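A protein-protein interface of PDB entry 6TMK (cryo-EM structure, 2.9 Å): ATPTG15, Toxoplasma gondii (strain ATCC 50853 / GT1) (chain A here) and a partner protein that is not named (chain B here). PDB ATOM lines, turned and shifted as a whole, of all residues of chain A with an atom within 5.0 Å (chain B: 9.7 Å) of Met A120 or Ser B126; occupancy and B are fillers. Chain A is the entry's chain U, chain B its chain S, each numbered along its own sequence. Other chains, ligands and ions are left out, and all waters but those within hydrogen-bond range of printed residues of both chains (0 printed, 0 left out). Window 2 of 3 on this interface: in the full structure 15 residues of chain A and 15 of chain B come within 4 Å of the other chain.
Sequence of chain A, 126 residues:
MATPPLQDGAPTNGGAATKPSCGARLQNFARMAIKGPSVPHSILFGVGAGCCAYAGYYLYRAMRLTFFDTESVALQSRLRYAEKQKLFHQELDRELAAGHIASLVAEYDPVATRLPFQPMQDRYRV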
ATOM      1  N   PRO A 110      -6.454   9.346  17.658  1.00  0.00           N
ATOM      2  CA  PRO A 110      -6.807  10.191  16.515  1.00  0.00           C
ATOM      3  C   PRO A 110      -6.174  11.567  16.537  1.00  0.00           C
ATOM      4  O   PRO A 110      -6.310  12.304  15.553  1.00  0.00           O
ATOM      5  CB  PRO A 110      -8.327  10.290  16.631  1.00  0.00           C
ATOM      6  CG  PRO A 110      -8.572  10.210  18.070  1.00  0.00           C
ATOM      7  CD  PRO A 110      -7.590   9.200  18.580  1.00  0.00           C
ATOM      8  N   VAL A 111      -5.490  11.936  17.617  1.00  0.00           N
ATOM      9  CA  VAL A 111      -4.823  13.229  17.662  1.00  0.00           C
ATOM     10  C   VAL A 111      -3.536  13.198  16.856  1.00  0.00           C
ATOM     11  O   VAL A 111      -3.104  14.227  16.328  1.00  0.00           O
ATOM     12  CB  VAL A 111      -4.559  13.634  19.119  1.00  0.00           C
ATOM     13  CG1 VAL A 111      -3.783  14.921  19.175  1.00  0.00           C
ATOM     14  CG2 VAL A 111      -5.858  13.769  19.862  1.00  0.00           C
ATOM     15  N   ARG A 114      -3.498  14.631  13.499  1.00  0.00           N
ATOM     16  CA  ARG A 114      -3.454  16.079  13.384  1.00  0.00           C
ATOM     17  C   ARG A 114      -2.123  16.537  12.809  1.00  0.00           C
ATOM     18  O   ARG A 114      -1.061  16.014  13.152  1.00  0.00           O
ATOM     19  CB  ARG A 114      -3.675  16.708  14.756  1.00  0.00           C
ATOM     20  CG  ARG A 114      -4.074  18.149  14.727  1.00  0.00           C
ATOM     21  CD  ARG A 114      -4.270  18.673  16.125  1.00  0.00           C
ATOM     22  NE  ARG A 114      -3.007  18.907  16.809  1.00  0.00           N
ATOM     23  CZ  ARG A 114      -2.327  20.045  16.755  1.00  0.00           C
ATOM     24  NH1 ARG A 114      -2.778  21.061  16.039  1.00  0.00           N
ATOM     25  NH2 ARG A 114      -1.186  20.165  17.411  1.00  0.00           N
ATOM     26  N   GLN A 118      -2.687  22.936  13.059  1.00  0.00           N
ATOM     27  CA  GLN A 118      -3.922  22.738  12.320  1.00  0.00           C
ATOM     28  C   GLN A 118      -4.956  22.166  13.273  1.00  0.00           C
ATOM     29  O   GLN A 118      -4.602  21.599  14.312  1.00  0.00           O
ATOM     30  CB  GLN A 118      -3.735  21.798  11.125  1.00  0.00           C
ATOM     31  CG  GLN A 118      -3.014  22.426   9.953  1.00  0.00           C
ATOM     32  CD  GLN A 118      -3.870  23.433   9.218  1.00  0.00           C
ATOM     33  OE1 GLN A 118      -4.854  23.075   8.571  1.00  0.00           O
ATOM     34  NE2 GLN A 118      -3.503  24.705   9.317  1.00  0.00           N
ATOM     35  N   PRO A 119      -6.236  22.297  12.951  1.00  0.00           N
ATOM     36  CA  PRO A 119      -7.270  21.733  13.815  1.00  0.00           C
ATOM     37  C   PRO A 119      -7.526  20.264  13.516  1.00  0.00           C
ATOM     38  O   PRO A 119      -7.249  19.753  12.430  1.00  0.00           O
ATOM     39  CB  PRO A 119      -8.497  22.582  13.480  1.00  0.00           C
ATOM     40  CG  PRO A 119      -8.306  22.917  12.056  1.00  0.00           C
ATOM     41  CD  PRO A 119      -6.821  23.097  11.862  1.00  0.00           C
ATOM     42  N   MET A 120      -8.068  19.589  14.520  1.00  0.00           N
ATOM     43  CA  MET A 120      -8.372  18.174  14.415  1.00  0.00           C
ATOM     44  C   MET A 120      -9.670  17.960  13.648  1.00  0.00           C
ATOM     45  O   MET A 120     -10.612  18.751  13.742  1.00  0.00           O
ATOM     46  CB  MET A 120      -8.474  17.556  15.804  1.00  0.00           C
ATOM     47  CG  MET A 120      -8.397  16.056  15.810  1.00  0.00           C
ATOM     48  SD  MET A 120      -8.881  15.367  17.395  1.00  0.00           S
ATOM     49  CE  MET A 120      -9.297  13.716  16.879  1.00  0.00           C
ATOM     50  N   GLN A 121      -9.711  16.876  12.881  1.00  0.00           N
ATOM     51  CA  GLN A 121     -10.854  16.559  12.038  1.00  0.00           C
ATOM     52  C   GLN A 121     -11.781  15.569  12.725  1.00  0.00           C
ATOM     53  O   GLN A 121     -11.332  14.575  13.302  1.00  0.00           O
ATOM     54  CB  GLN A 121     -10.397  15.975  10.705  1.00  0.00           C
ATOM     55  CG  GLN A 121      -9.569  16.913   9.866  1.00  0.00           C
ATOM     56  CD  GLN A 121      -9.206  16.313   8.527  1.00  0.00           C
ATOM     57  OE1 GLN A 121     -10.078  15.957   7.735  1.00  0.00           O
ATOM     58  NE2 GLN A 121      -7.916  16.185   8.272  1.00  0.00           N
ATOM     59  N   ASP A 122     -13.083  15.843  12.647  1.00  0.00           N
ATOM     60  CA  ASP A 122     -14.087  14.917  13.149  1.00  0.00           C
ATOM     61  C   ASP A 122     -14.176  13.655  12.308  1.00  0.00           C
ATOM     62  O   ASP A 122     -14.796  12.679  12.744  1.00  0.00           O
ATOM     63  CB  ASP A 122     -15.454  15.601  13.189  1.00  0.00           C
ATOM     64  CG  ASP A 122     -15.648  16.449  14.430  1.00  0.00           C
ATOM     65  OD1 ASP A 122     -14.660  16.682  15.157  1.00  0.00           O
ATOM     66  OD2 ASP A 122     -16.791  16.886  14.678  1.00  0.00           O
ATOM     67  N   TYR A 124     -11.830  11.598  11.904  1.00  0.00           N
ATOM     68  CA  TYR A 124     -11.180  10.575  12.719  1.00  0.00           C
ATOM     69  C   TYR A 124     -11.803  10.499  14.109  1.00  0.00           C
ATOM     70  O   TYR A 124     -11.115  10.448  15.125  1.00  0.00           O
ATOM     71  CB  TYR A 124      -9.688  10.862  12.806  1.00  0.00           C
ATOM     72  CG  TYR A 124      -8.985  10.982  11.474  1.00  0.00           C
ATOM     73  CD1 TYR A 124      -8.486   9.868  10.827  1.00  0.00           C
ATOM     74  CD2 TYR A 124      -8.817  12.211  10.867  1.00  0.00           C
ATOM     75  CE1 TYR A 124      -7.844   9.974   9.618  1.00  0.00           C
ATOM     76  CE2 TYR A 124      -8.173  12.324   9.656  1.00  0.00           C
ATOM     77  CZ  TYR A 124      -7.690  11.200   9.038  1.00  0.00           C
ATOM     78  OH  TYR A 124      -7.047  11.296   7.829  1.00  0.00           O
ATOM     79  N   VAL A 126     -13.581  12.053  16.643  1.00  0.00           N
ATOM     80  CA  VAL A 126     -13.279  12.790  17.864  1.00  0.00           C
ATOM     81  C   VAL A 126     -14.075  12.205  19.028  1.00  0.00           C
ATOM     82  O   VAL A 126     -15.264  11.907  18.905  1.00  0.00           O
ATOM     83  CB  VAL A 126     -13.580  14.286  17.715  1.00  0.00           C
ATOM     84  CG1 VAL A 126     -13.446  14.978  19.056  1.00  0.00           C
ATOM     85  CG2 VAL A 126     -12.651  14.917  16.711  1.00  0.00           C
ATOM     86  OXT VAL A 126     -13.541  12.015  20.122  1.00  0.00           O
ATOM     87  N   PRO B 119     -20.124  12.594  14.151  1.00  0.00           N
ATOM     88  CA  PRO B 119     -20.174  11.577  15.205  1.00  0.00           C
ATOM     89  C   PRO B 119     -21.364  11.771  16.127  1.00  0.00           C
ATOM     90  O   PRO B 119     -21.764  12.898  16.435  1.00  0.00           O
ATOM     91  CB  PRO B 119     -18.852  11.786  15.952  1.00  0.00           C
ATOM     92  CG  PRO B 119     -18.511  13.195  15.704  1.00  0.00           C
ATOM     93  CD  PRO B 119     -18.955  13.472  14.305  1.00  0.00           C
ATOM     94  N   LEU B 122     -19.578  13.474  20.563  1.00  0.00           N
ATOM     95  CA  LEU B 122     -18.344  14.239  20.426  1.00  0.00           C
ATOM     96  C   LEU B 122     -17.636  14.223  21.776  1.00  0.00           C
ATOM     97  O   LEU B 122     -18.105  14.836  22.740  1.00  0.00           O
ATOM     98  CB  LEU B 122     -18.645  15.657  19.956  1.00  0.00           C
ATOM     99  CG  LEU B 122     -17.452  16.487  19.491  1.00  0.00           C
ATOM    100  CD1 LEU B 122     -17.901  17.427  18.392  1.00  0.00           C
ATOM    101  CD2 LEU B 122     -16.818  17.261  20.637  1.00  0.00           C
ATOM    102  N   LEU B 123     -16.503  13.526  21.842  1.00  0.00           N
ATOM    103  CA  LEU B 123     -15.833  13.233  23.103  1.00  0.00           C
ATOM    104  C   LEU B 123     -14.437  13.830  23.151  1.00  0.00           C
ATOM    105  O   LEU B 123     -13.469  13.139  23.481  1.00  0.00           O
ATOM    106  CB  LEU B 123     -15.751  11.725  23.317  1.00  0.00           C
ATOM    107  CG  LEU B 123     -17.079  11.007  23.499  1.00  0.00           C
ATOM    108  CD1 LEU B 123     -16.857   9.522  23.490  1.00  0.00           C
ATOM    109  CD2 LEU B 123     -17.734  11.441  24.788  1.00  0.00           C
ATOM    110  N   GLY B 124     -14.323  15.106  22.815  1.00  0.00           N
ATOM    111  CA  GLY B 124     -13.092  15.827  22.998  1.00  0.00           C
ATOM    112  C   GLY B 124     -13.037  17.058  22.124  1.00  0.00           C
ATOM    113  O   GLY B 124     -13.818  17.218  21.182  1.00  0.00           O
ATOM    114  N   PRO B 125     -12.111  17.956  22.424  1.00  0.00           N
ATOM    115  CA  PRO B 125     -11.980  19.181  21.635  1.00  0.00           C
ATOM    116  C   PRO B 125     -11.242  18.933  20.327  1.00  0.00           C
ATOM    117  O   PRO B 125     -10.605  17.902  20.114  1.00  0.00           O
ATOM    118  CB  PRO B 125     -11.180  20.104  22.557  1.00  0.00           C
ATOM    119  CG  PRO B 125     -10.355  19.178  23.369  1.00  0.00           C
ATOM    120  CD  PRO B 125     -11.174  17.930  23.559  1.00  0.00           C
ATOM    121  N   SER B 126     -11.351  19.918  19.440  1.00  0.00           N
ATOM    122  CA  SER B 126     -10.636  19.932  18.163  1.00  0.00           C
ATOM    123  C   SER B 126     -10.121  21.357  17.989  1.00  0.00           C
ATOM    124  O   SER B 126     -10.801  22.214  17.417  1.00  0.00           O
ATOM    125  CB  SER B 126     -11.534  19.504  17.014  1.00  0.00           C
ATOM    126  OG  SER B 126     -12.129  18.245  17.275  1.00  0.00           O
ATOM    127  N   THR B 127      -8.915  21.600  18.488  1.00  0.00           N
ATOM    128  CA  THR B 127      -8.358  22.944  18.542  1.00  0.00           C
ATOM    129  C   THR B 127      -7.289  23.139  17.475  1.00  0.00           C
ATOM    130  O   THR B 127      -7.473  23.910  16.534  1.00  0.00           O
ATOM    131  CB  THR B 127      -7.756  23.233  19.927  1.00  0.00           C
ATOM    132  OG1 THR B 127      -6.663  22.341  20.171  1.00  0.00           O
ATOM    133  CG2 THR B 127      -8.800  23.033  21.008  1.00  0.00           C
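Of the 10 printed residues of chain A, 4 touch a printed residue of chain B. Printed residues of chain A that touch a printed residue of chain B: Pro A119, Met A120, Asp A122 and Val A126. Hydrophobic or aromatic side chains of chain A that line the printed part of chain B: Pro A119, Met A120 and Val A126. Of the 7 printed residues of chain B, 5 touch a printed residue of chain A. Hydrophobic or aromatic side chains of chain B within 4 Å of the printed part of chain A: Leu B122 and Leu B123. Among the printed residues, 7 pairs touch across the chains.
No residue of chain B comes within 4 Å of Pro A110. Arg A114 touches none of the printed residues of chain B. Of the printed residues of chain B, Pro A119 touches Thr B127 (3.5 Å). Met A120 touches one residue of chain B. Of the printed residues of chain B, Asp A122 touches Leu B122 (3.9 Å) and Ser B126 (3.7 Å). Of the printed residues of chain A, Gly B124 touches Val A126. Pro B125 touches none of the printed residues of chain A. Ser B126 touches just these residues of chain A: Met A120 (3.5 Å), Asp A122 (3.7 Å) and Val A126 (3.4 Å). The nearest residue of chain B that does not touch Met A120 is Pro B125 (4.1 Å). The nearest printed residue of chain B that does not touch Val A126 is Leu B122 (4.2 Å).
Among the printed residues, merely in contact across the chains: Val A126 with Gly B124 (3.1 Å), Val A126 with Ser B126 (3.4 Å), Met A120 with Ser B126 (3.5 Å), Pro A119 with Thr B127 (3.5 Å), Val A126 with Leu B123 (3.5 Å), Asp A122 with Ser B126 (3.7 Å) and Asp A122 with Leu B122 (3.9 Å).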
